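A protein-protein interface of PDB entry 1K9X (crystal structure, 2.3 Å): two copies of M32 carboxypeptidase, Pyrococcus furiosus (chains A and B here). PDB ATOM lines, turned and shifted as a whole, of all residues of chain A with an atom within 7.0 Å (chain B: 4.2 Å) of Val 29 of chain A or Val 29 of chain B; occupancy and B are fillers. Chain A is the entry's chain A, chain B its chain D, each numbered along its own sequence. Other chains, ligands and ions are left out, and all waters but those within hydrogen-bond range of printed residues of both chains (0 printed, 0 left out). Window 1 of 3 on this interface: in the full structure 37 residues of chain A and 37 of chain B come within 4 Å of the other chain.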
ATOM      1  N   ILE A  23      24.252 -13.626   5.474  1.00  0.00           N
ATOM      2  CA  ILE A  23      24.807 -13.959   6.781  1.00  0.00           C
ATOM      3  C   ILE A  23      23.738 -14.547   7.702  1.00  0.00           C
ATOM      4  O   ILE A  23      24.011 -15.456   8.504  1.00  0.00           O
ATOM      5  CB  ILE A  23      25.452 -12.711   7.413  1.00  0.00           C
ATOM      6  CG1 ILE A  23      26.615 -12.263   6.524  1.00  0.00           C
ATOM      7  CG2 ILE A  23      25.943 -13.021   8.835  1.00  0.00           C
ATOM      8  CD1 ILE A  23      27.294 -11.000   6.969  1.00  0.00           C
ATOM      9  N   GLY A  24      22.515 -14.033   7.571  1.00  0.00           N
ATOM     10  CA  GLY A  24      21.407 -14.523   8.373  1.00  0.00           C
ATOM     11  C   GLY A  24      21.088 -15.946   7.967  1.00  0.00           C
ATOM     12  O   GLY A  24      20.716 -16.783   8.790  1.00  0.00           O
ATOM     13  N   HIS A  25      21.232 -16.222   6.679  1.00  0.00           N
ATOM     14  CA  HIS A  25      20.978 -17.557   6.170  1.00  0.00           C
ATOM     15  C   HIS A  25      22.018 -18.467   6.815  1.00  0.00           C
ATOM     16  O   HIS A  25      21.694 -19.520   7.365  1.00  0.00           O
ATOM     17  CB  HIS A  25      21.125 -17.573   4.654  1.00  0.00           C
ATOM     18  CG  HIS A  25      20.949 -18.929   4.037  1.00  0.00           C
ATOM     19  ND1 HIS A  25      19.711 -19.466   3.753  1.00  0.00           N
ATOM     20  CD2 HIS A  25      21.861 -19.843   3.626  1.00  0.00           C
ATOM     21  CE1 HIS A  25      19.872 -20.651   3.188  1.00  0.00           C
ATOM     22  NE2 HIS A  25      21.166 -20.902   3.099  1.00  0.00           N
ATOM     23  N   ALA A  26      23.274 -18.047   6.743  1.00  0.00           N
ATOM     24  CA  ALA A  26      24.363 -18.799   7.335  1.00  0.00           C
ATOM     25  C   ALA A  26      24.088 -18.982   8.837  1.00  0.00           C
ATOM     26  O   ALA A  26      24.118 -20.098   9.346  1.00  0.00           O
ATOM     27  CB  ALA A  26      25.667 -18.060   7.120  1.00  0.00           C
ATOM     28  N   GLN A  27      23.804 -17.886   9.537  1.00  0.00           N
ATOM     29  CA  GLN A  27      23.526 -17.949  10.971  1.00  0.00           C
ATOM     30  C   GLN A  27      22.413 -18.938  11.305  1.00  0.00           C
ATOM     31  O   GLN A  27      22.499 -19.639  12.313  1.00  0.00           O
ATOM     32  CB  GLN A  27      23.140 -16.575  11.503  1.00  0.00           C
ATOM     33  CG  GLN A  27      24.264 -15.562  11.552  1.00  0.00           C
ATOM     34  CD  GLN A  27      25.113 -15.675  12.810  1.00  0.00           C
ATOM     35  OE1 GLN A  27      25.758 -14.706  13.215  1.00  0.00           O
ATOM     36  NE2 GLN A  27      25.125 -16.856  13.425  1.00  0.00           N
ATOM     37  N   SER A  28      21.378 -18.991  10.467  1.00  0.00           N
ATOM     38  CA  SER A  28      20.253 -19.906  10.678  1.00  0.00           C
ATOM     39  C   SER A  28      20.699 -21.349  10.556  1.00  0.00           C
ATOM     40  O   SER A  28      20.250 -22.209  11.312  1.00  0.00           O
ATOM     41  CB  SER A  28      19.137 -19.670   9.645  1.00  0.00           C
ATOM     42  OG  SER A  28      18.540 -18.397   9.788  1.00  0.00           O
ATOM     43  N   VAL A  29      21.557 -21.618   9.571  1.00  0.00           N
ATOM     44  CA  VAL A  29      22.055 -22.962   9.348  1.00  0.00           C
ATOM     45  C   VAL A  29      22.932 -23.365  10.529  1.00  0.00           C
ATOM     46  O   VAL A  29      22.798 -24.459  11.071  1.00  0.00           O
ATOM     47  CB  VAL A  29      22.858 -23.038   8.029  1.00  0.00           C
ATOM     48  CG1 VAL A  29      23.368 -24.453   7.811  1.00  0.00           C
ATOM     49  CG2 VAL A  29      21.959 -22.629   6.845  1.00  0.00           C
ATOM     50  N   LEU A  30      23.823 -22.474  10.939  1.00  0.00           N
ATOM     51  CA  LEU A  30      24.686 -22.753  12.080  1.00  0.00           C
ATOM     52  C   LEU A  30      23.844 -22.993  13.330  1.00  0.00           C
ATOM     53  O   LEU A  30      24.154 -23.868  14.139  1.00  0.00           O
ATOM     54  CB  LEU A  30      25.647 -21.581  12.320  1.00  0.00           C
ATOM     55  CG  LEU A  30      26.905 -21.539  11.446  1.00  0.00           C
ATOM     56  CD1 LEU A  30      26.534 -21.800   9.992  1.00  0.00           C
ATOM     57  CD2 LEU A  30      27.593 -20.187  11.602  1.00  0.00           C
ATOM     58  N   GLY A  31      22.768 -22.224  13.474  1.00  0.00           N
ATOM     59  CA  GLY A  31      21.914 -22.365  14.639  1.00  0.00           C
ATOM     60  C   GLY A  31      21.174 -23.678  14.645  1.00  0.00           C
ATOM     61  O   GLY A  31      21.125 -24.370  15.656  1.00  0.00           O
ATOM     62  N   TRP A  32      20.607 -24.022  13.499  1.00  0.00           N
ATOM     63  CA  TRP A  32      19.861 -25.256  13.346  1.00  0.00           C
ATOM     64  C   TRP A  32      20.761 -26.471  13.526  1.00  0.00           C
ATOM     65  O   TRP A  32      20.436 -27.383  14.282  1.00  0.00           O
ATOM     66  CB  TRP A  32      19.210 -25.295  11.963  1.00  0.00           C
ATOM     67  CG  TRP A  32      18.522 -26.582  11.663  1.00  0.00           C
ATOM     68  CD1 TRP A  32      17.283 -26.965  12.071  1.00  0.00           C
ATOM     69  CD2 TRP A  32      19.058 -27.681  10.919  1.00  0.00           C
ATOM     70  NE1 TRP A  32      17.008 -28.236  11.628  1.00  0.00           N
ATOM     71  CE2 TRP A  32      18.086 -28.697  10.916  1.00  0.00           C
ATOM     72  CE3 TRP A  32      20.271 -27.904  10.254  1.00  0.00           C
ATOM     73  CZ2 TRP A  32      18.286 -29.923  10.279  1.00  0.00           C
ATOM     74  CZ3 TRP A  32      20.471 -29.120   9.619  1.00  0.00           C
ATOM     75  CH2 TRP A  32      19.485 -30.113   9.635  1.00  0.00           C
ATOM     76  N   ASP A  33      21.891 -26.479  12.823  1.00  0.00           N
ATOM     77  CA  ASP A  33      22.842 -27.586  12.901  1.00  0.00           C
ATOM     78  C   ASP A  33      23.337 -27.821  14.319  1.00  0.00           C
ATOM     79  O   ASP A  33      23.477 -28.962  14.752  1.00  0.00           O
ATOM     80  CB  ASP A  33      24.045 -27.326  11.993  1.00  0.00           C
ATOM     81  CG  ASP A  33      25.109 -28.405  12.120  1.00  0.00           C
ATOM     82  OD1 ASP A  33      26.034 -28.251  12.946  1.00  0.00           O
ATOM     83  OD2 ASP A  33      25.001 -29.424  11.408  1.00  0.00           O
ATOM     84  N   LEU A  34      23.615 -26.734  15.028  1.00  0.00           N
ATOM     85  CA  LEU A  34      24.090 -26.823  16.396  1.00  0.00           C
ATOM     86  C   LEU A  34      23.129 -27.653  17.253  1.00  0.00           C
ATOM     87  O   LEU A  34      23.565 -28.517  18.008  1.00  0.00           O
ATOM     88  CB  LEU A  34      24.286 -25.411  16.966  1.00  0.00           C
ATOM     89  CG  LEU A  34      24.335 -25.106  18.472  1.00  0.00           C
ATOM     90  CD1 LEU A  34      24.914 -26.251  19.270  1.00  0.00           C
ATOM     91  CD2 LEU A  34      25.152 -23.839  18.677  1.00  0.00           C
ATOM     92  N   GLU A  35      21.830 -27.420  17.103  1.00  0.00           N
ATOM     93  CA  GLU A  35      20.823 -28.151  17.871  1.00  0.00           C
ATOM     94  C   GLU A  35      20.507 -29.556  17.353  1.00  0.00           C
ATOM     95  O   GLU A  35      20.146 -30.447  18.132  1.00  0.00           O
ATOM     96  CB  GLU A  35      19.508 -27.361  17.907  1.00  0.00           C
ATOM     97  CG  GLU A  35      19.519 -26.145  18.813  1.00  0.00           C
ATOM     98  CD  GLU A  35      19.887 -26.504  20.244  1.00  0.00           C
ATOM     99  OE1 GLU A  35      19.235 -27.390  20.842  1.00  0.00           O
ATOM    100  OE2 GLU A  35      20.836 -25.897  20.765  1.00  0.00           O
ATOM    101  N   ARG A  46      31.972 -23.449  16.782  1.00  0.00           N
ATOM    102  CA  ARG A  46      30.733 -22.917  16.240  1.00  0.00           C
ATOM    103  C   ARG A  46      30.474 -21.556  16.912  1.00  0.00           C
ATOM    104  O   ARG A  46      30.102 -20.588  16.250  1.00  0.00           O
ATOM    105  CB  ARG A  46      29.573 -23.882  16.511  1.00  0.00           C
ATOM    106  CG  ARG A  46      28.211 -23.352  16.101  1.00  0.00           C
ATOM    107  CD  ARG A  46      28.099 -23.143  14.600  1.00  0.00           C
ATOM    108  NE  ARG A  46      27.498 -24.290  13.924  1.00  0.00           N
ATOM    109  CZ  ARG A  46      28.171 -25.336  13.459  1.00  0.00           C
ATOM    110  NH1 ARG A  46      29.484 -25.401  13.578  1.00  0.00           N
ATOM    111  NH2 ARG A  46      27.524 -26.331  12.885  1.00  0.00           N
ATOM    112  N   GLN A  50      29.778 -17.984  15.132  1.00  0.00           N
ATOM    113  CA  GLN A  50      28.523 -17.248  15.275  1.00  0.00           C
ATOM    114  C   GLN A  50      28.785 -15.832  15.786  1.00  0.00           C
ATOM    115  O   GLN A  50      28.170 -14.861  15.321  1.00  0.00           O
ATOM    116  CB  GLN A  50      27.588 -17.982  16.241  1.00  0.00           C
ATOM    117  CG  GLN A  50      27.144 -19.339  15.748  1.00  0.00           C
ATOM    118  CD  GLN A  50      26.292 -20.067  16.758  1.00  0.00           C
ATOM    119  OE1 GLN A  50      26.743 -20.361  17.865  1.00  0.00           O
ATOM    120  NE2 GLN A  50      25.054 -20.364  16.384  1.00  0.00           N
ATOM    121  N   THR A 242      12.941 -22.765  12.219  1.00  0.00           N
ATOM    122  CA  THR A 242      13.990 -21.944  11.631  1.00  0.00           C
ATOM    123  C   THR A 242      13.729 -21.752  10.148  1.00  0.00           C
ATOM    124  O   THR A 242      13.416 -22.700   9.433  1.00  0.00           O
ATOM    125  CB  THR A 242      15.389 -22.581  11.800  1.00  0.00           C
ATOM    126  OG1 THR A 242      15.638 -22.839  13.190  1.00  0.00           O
ATOM    127  CG2 THR A 242      16.462 -21.631  11.284  1.00  0.00           C
ATOM    128  N   GLU A 243      13.857 -20.512   9.696  1.00  0.00           N
ATOM    129  CA  GLU A 243      13.637 -20.174   8.301  1.00  0.00           C
ATOM    130  C   GLU A 243      14.977 -19.932   7.607  1.00  0.00           C
ATOM    131  O   GLU A 243      15.656 -18.945   7.891  1.00  0.00           O
ATOM    132  CB  GLU A 243      12.767 -18.907   8.205  1.00  0.00           C
ATOM    133  CG  GLU A 243      12.397 -18.479   6.786  1.00  0.00           C
ATOM    134  CD  GLU A 243      12.692 -17.003   6.502  1.00  0.00           C
ATOM    135  OE1 GLU A 243      12.429 -16.149   7.386  1.00  0.00           O
ATOM    136  OE2 GLU A 243      13.172 -16.693   5.384  1.00  0.00           O
ATOM    137  N   PHE A 244      15.361 -20.840   6.712  1.00  0.00           N
ATOM    138  CA  PHE A 244      16.601 -20.689   5.956  1.00  0.00           C
ATOM    139  C   PHE A 244      16.279 -19.791   4.770  1.00  0.00           C
ATOM    140  O   PHE A 244      17.070 -18.935   4.363  1.00  0.00           O
ATOM    141  CB  PHE A 244      17.088 -22.039   5.424  1.00  0.00           C
ATOM    142  CG  PHE A 244      17.746 -22.916   6.456  1.00  0.00           C
ATOM    143  CD1 PHE A 244      18.434 -24.061   6.061  1.00  0.00           C
ATOM    144  CD2 PHE A 244      17.685 -22.605   7.814  1.00  0.00           C
ATOM    145  CE1 PHE A 244      19.053 -24.880   6.998  1.00  0.00           C
ATOM    146  CE2 PHE A 244      18.302 -23.420   8.761  1.00  0.00           C
ATOM    147  CZ  PHE A 244      18.988 -24.561   8.352  1.00  0.00           C
ATOM    148  N   ASP A 248      12.815 -23.199   2.162  1.00  0.00           N
ATOM    149  CA  ASP A 248      13.477 -24.160   3.041  1.00  0.00           C
ATOM    150  C   ASP A 248      13.200 -23.765   4.491  1.00  0.00           C
ATOM    151  O   ASP A 248      13.938 -22.979   5.091  1.00  0.00           O
ATOM    152  CB  ASP A 248      14.984 -24.167   2.773  1.00  0.00           C
ATOM    153  CG  ASP A 248      15.731 -25.186   3.630  1.00  0.00           C
ATOM    154  OD1 ASP A 248      15.126 -25.757   4.558  1.00  0.00           O
ATOM    155  OD2 ASP A 248      16.934 -25.413   3.377  1.00  0.00           O
ATOM    156  N   ARG A 250      12.486 -25.334   8.282  1.00  0.00           N
ATOM    157  CA  ARG A 250      12.571 -26.551   9.079  1.00  0.00           C
ATOM    158  C   ARG A 250      12.024 -26.408  10.492  1.00  0.00           C
ATOM    159  O   ARG A 250      12.007 -25.316  11.064  1.00  0.00           O
ATOM    160  CB  ARG A 250      14.027 -27.026   9.128  1.00  0.00           C
ATOM    161  CG  ARG A 250      14.693 -27.028   7.751  1.00  0.00           C
ATOM    162  CD  ARG A 250      16.147 -27.464   7.784  1.00  0.00           C
ATOM    163  NE  ARG A 250      16.796 -27.210   6.497  1.00  0.00           N
ATOM    164  CZ  ARG A 250      18.039 -27.574   6.194  1.00  0.00           C
ATOM    165  NH1 ARG A 250      18.777 -28.225   7.080  1.00  0.00           N
ATOM    166  NH2 ARG A 250      18.559 -27.250   5.016  1.00  0.00           N
ATOM    167  N   HIS B  25      33.701 -21.311   8.015  1.00  0.00           N
ATOM    168  CA  HIS B  25      32.978 -22.280   8.837  1.00  0.00           C
ATOM    169  C   HIS B  25      31.530 -22.349   8.336  1.00  0.00           C
ATOM    170  O   HIS B  25      30.957 -23.435   8.161  1.00  0.00           O
ATOM    171  CB  HIS B  25      33.041 -21.815  10.291  1.00  0.00           C
ATOM    172  CG  HIS B  25      32.339 -22.708  11.261  1.00  0.00           C
ATOM    173  ND1 HIS B  25      32.949 -23.798  11.847  1.00  0.00           N
ATOM    174  CD2 HIS B  25      31.096 -22.639  11.797  1.00  0.00           C
ATOM    175  CE1 HIS B  25      32.112 -24.358  12.703  1.00  0.00           C
ATOM    176  NE2 HIS B  25      30.981 -23.673  12.691  1.00  0.00           N
ATOM    177  N   ALA B  26      30.951 -21.176   8.083  1.00  0.00           N
ATOM    178  CA  ALA B  26      29.581 -21.079   7.574  1.00  0.00           C
ATOM    179  C   ALA B  26      29.471 -21.820   6.239  1.00  0.00           C
ATOM    180  O   ALA B  26      28.591 -22.660   6.063  1.00  0.00           O
ATOM    181  CB  ALA B  26      29.194 -19.615   7.405  1.00  0.00           C
ATOM    182  N   GLN B  27      30.373 -21.514   5.308  1.00  0.00           N
ATOM    183  CA  GLN B  27      30.397 -22.163   3.987  1.00  0.00           C
ATOM    184  C   GLN B  27      30.446 -23.688   4.087  1.00  0.00           C
ATOM    185  O   GLN B  27      29.669 -24.391   3.428  1.00  0.00           O
ATOM    186  CB  GLN B  27      31.614 -21.694   3.182  1.00  0.00           C
ATOM    187  CG  GLN B  27      31.543 -20.274   2.633  1.00  0.00           C
ATOM    188  CD  GLN B  27      30.671 -20.146   1.383  1.00  0.00           C
ATOM    189  OE1 GLN B  27      30.907 -19.268   0.544  1.00  0.00           O
ATOM    190  NE2 GLN B  27      29.658 -21.009   1.255  1.00  0.00           N
ATOM    191  N   SER B  28      31.365 -24.206   4.897  1.00  0.00           N
ATOM    192  CA  SER B  28      31.485 -25.653   5.057  1.00  0.00           C
ATOM    193  C   SER B  28      30.156 -26.271   5.500  1.00  0.00           C
ATOM    194  O   SER B  28      29.753 -27.339   5.018  1.00  0.00           O
ATOM    195  CB  SER B  28      32.582 -25.996   6.081  1.00  0.00           C
ATOM    196  OG  SER B  28      33.872 -25.639   5.616  1.00  0.00           O
ATOM    197  N   VAL B  29      29.469 -25.600   6.419  1.00  0.00           N
ATOM    198  CA  VAL B  29      28.195 -26.108   6.914  1.00  0.00           C
ATOM    199  C   VAL B  29      27.139 -25.968   5.833  1.00  0.00           C
ATOM    200  O   VAL B  29      26.297 -26.849   5.648  1.00  0.00           O
ATOM    201  CB  VAL B  29      27.746 -25.348   8.164  1.00  0.00           C
ATOM    202  CG1 VAL B  29      26.437 -25.942   8.704  1.00  0.00           C
ATOM    203  CG2 VAL B  29      28.848 -25.413   9.208  1.00  0.00           C
ATOM    204  N   LEU B  30      27.180 -24.857   5.117  1.00  0.00           N
ATOM    205  CA  LEU B  30      26.230 -24.633   4.029  1.00  0.00           C
ATOM    206  C   LEU B  30      26.378 -25.732   2.973  1.00  0.00           C
ATOM    207  O   LEU B  30      25.386 -26.267   2.475  1.00  0.00           O
ATOM    208  CB  LEU B  30      26.490 -23.268   3.379  1.00  0.00           C
ATOM    209  CG  LEU B  30      25.639 -22.046   3.733  1.00  0.00           C
ATOM    210  CD1 LEU B  30      24.710 -22.313   4.904  1.00  0.00           C
ATOM    211  CD2 LEU B  30      26.580 -20.906   4.018  1.00  0.00           C
ATOM    212  N   GLY B  31      27.623 -26.065   2.640  1.00  0.00           N
ATOM    213  CA  GLY B  31      27.883 -27.089   1.637  1.00  0.00           C
ATOM    214  C   GLY B  31      27.536 -28.476   2.133  1.00  0.00           C
ATOM    215  O   GLY B  31      26.902 -29.262   1.437  1.00  0.00           O
ATOM    216  N   TRP B  32      27.952 -28.780   3.352  1.00  0.00           N
ATOM    217  CA  TRP B  32      27.659 -30.075   3.935  1.00  0.00           C
ATOM    218  C   TRP B  32      26.137 -30.264   3.924  1.00  0.00           C
ATOM    219  O   TRP B  32      25.621 -31.230   3.361  1.00  0.00           O
ATOM    220  CB  TRP B  32      28.208 -30.137   5.372  1.00  0.00           C
ATOM    221  CG  TRP B  32      27.856 -31.400   6.097  1.00  0.00           C
ATOM    222  CD1 TRP B  32      28.439 -32.627   5.944  1.00  0.00           C
ATOM    223  CD2 TRP B  32      26.768 -31.585   7.016  1.00  0.00           C
ATOM    224  NE1 TRP B  32      27.777 -33.561   6.701  1.00  0.00           N
ATOM    225  CE2 TRP B  32      26.748 -32.950   7.370  1.00  0.00           C
ATOM    226  CE3 TRP B  32      25.805 -30.724   7.570  1.00  0.00           C
ATOM    227  CZ2 TRP B  32      25.804 -33.485   8.255  1.00  0.00           C
ATOM    228  CZ3 TRP B  32      24.859 -31.258   8.459  1.00  0.00           C
ATOM    229  CH2 TRP B  32      24.869 -32.626   8.788  1.00  0.00           C
ATOM    230  N   ASP B  33      25.420 -29.317   4.521  1.00  0.00           N
ATOM    231  CA  ASP B  33      23.961 -29.405   4.583  1.00  0.00           C
ATOM    232  C   ASP B  33      23.290 -29.532   3.216  1.00  0.00           C
ATOM    233  O   ASP B  33      22.276 -30.218   3.075  1.00  0.00           O
ATOM    234  CB  ASP B  33      23.397 -28.188   5.317  1.00  0.00           C
ATOM    235  CG  ASP B  33      21.897 -28.257   5.475  1.00  0.00           C
ATOM    236  OD1 ASP B  33      21.183 -27.586   4.699  1.00  0.00           O
ATOM    237  OD2 ASP B  33      21.429 -28.998   6.368  1.00  0.00           O
ATOM    238  N   PHE B 244      34.538 -28.569   9.844  1.00  0.00           N
ATOM    239  CA  PHE B 244      33.876 -27.396  10.387  1.00  0.00           C
ATOM    240  C   PHE B 244      34.840 -26.778  11.379  1.00  0.00           C
ATOM    241  O   PHE B 244      34.811 -25.574  11.626  1.00  0.00           O
ATOM    242  CB  PHE B 244      32.569 -27.780  11.092  1.00  0.00           C
ATOM    243  CG  PHE B 244      31.489 -28.255  10.162  1.00  0.00           C
ATOM    244  CD1 PHE B 244      30.171 -28.332  10.596  1.00  0.00           C
ATOM    245  CD2 PHE B 244      31.782 -28.626   8.846  1.00  0.00           C
ATOM    246  CE1 PHE B 244      29.156 -28.770   9.741  1.00  0.00           C
ATOM    247  CE2 PHE B 244      30.770 -29.068   7.985  1.00  0.00           C
ATOM    248  CZ  PHE B 244      29.454 -29.138   8.439  1.00  0.00           C
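The guanidinium group (NH1) of Arg 46 of chain A sits at hydrogen-bond distance from a ring nitrogen (NE2) of His 25 of chain B, 2.5 Å away.
NH2 of Arg 250 of chain A is in salt-bridge range of OD1 of Asp 33 of chain B, at 2.7 Å.
ND1 of His 25 of chain A sits at hydrogen-bond distance from O of Phe 244 of chain A, 2.8 Å away.
The guanidinium group of Arg 46 of chain A sits at hydrogen-bond distance from the backbone carbonyl oxygen of Leu 30 of chain A, 3.4 Å away.
The side-chain carboxylate (OD1) of Asp 33 of chain A lies within salt-bridge range of the guanidinium group (NH2) of Arg 46 of chain A (2.4 Å).
The backbone NH (N) of Thr 242 of chain A sits at hydrogen-bond distance from the backbone carbonyl oxygen (O) of Arg 250 of chain A, 3.0 Å away.
The side-chain carboxylate of Asp 248 of chain A lies within salt-bridge range of the guanidinium group of Arg 250 of chain A, at 2.9 Å.
The backbone carbonyl oxygen (O) of Phe 244 of chain B sits at hydrogen-bond distance from a ring nitrogen (ND1) of His 25 of chain B, 2.6 Å away.
Leu 30 of chain B touches His 25 of chain A (CD1 to CD2, 3.98 Å).
Ala 26 of chain B touches Ala 26 of chain A.
CG1 of Val 29 of chain B touches CG1 of Val 29 of chain A (3.5 Å).
Leu 30 of chain B touches Val 29 of chain A.
CD1 of Leu 30 of chain A touches CA of Ala 26 of chain B, 3.96 Å away.
Asp 33 of chain B touches Trp 32 of chain A (OD2 to CZ3, 3.4 Å).
Asp 33 of chain A touches Trp 32 of chain B (OD2 to CZ3, 3.5 Å).
Printed residues of chain B within 4 Å of Val 29 of chain A: Val 29 (3.5 Å) and Leu 30 (3.4 Å).
Printed residues of chain A within 4 Å of Val 29 of chain B: Val 29.
Printed residues of chain B within 4 Å of Ala 26 of chain A: Ala 26.
Printed residues of chain B within 4 Å of Arg 250 of chain A: Asp 33.
Of the printed residues of chain A, His 25 of chain B touches Arg 46.
Of the printed residues of chain A, Trp 32 of chain B touches Asp 33 (3.5 Å).
The nearest printed residue of chain B that does not touch His 25 of chain A is Asp 33 of chain B (6.9 Å).
Of the 20 printed residues of chain A, 8 touch a printed residue of chain B.
Printed residues of chain B that touch a printed residue of chain A: His 25, Ala 26, Val 29, Leu 30, Trp 32 and Asp 33.
Hydrophobic or aromatic side chains of chain B within 4 Å of the printed part of chain A: His 25, Ala 26, Val 29, Leu 30 and Trp 32.
Among the printed residues, 9 pairs touch across the chains.
Among the printed residues, Asp or Glu carboxylates within 4 Å of a Lys or Arg side-chain nitrogen of the other chain: Arg 250 of chain A with Asp 33 of chain B (2.7 Å).
Ala 26 of chain B touches its own counterpart, Ala 26 of chain A.
Val 29 of chain B touches its own counterpart, Val 29 of chain A.
Val 29 of chain A touches Leu 30 of chain B, but with the chains exchanged Leu 30 of chain A does not touch Val 29 of chain B (4.2 Å).
Leu 30 of chain A touches Ala 26 of chain B, but with the chains exchanged Ala 26 of chain A does not touch Leu 30 of chain B (4.3 Å).
Positions printed for both chains: 25, 26, 27, 28, 29, 30, 31, 32, 33 and 244.
Of the 9 pairs that touch across the chains among the printed residues, 4 have their exchanged pair printed and touching as well.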
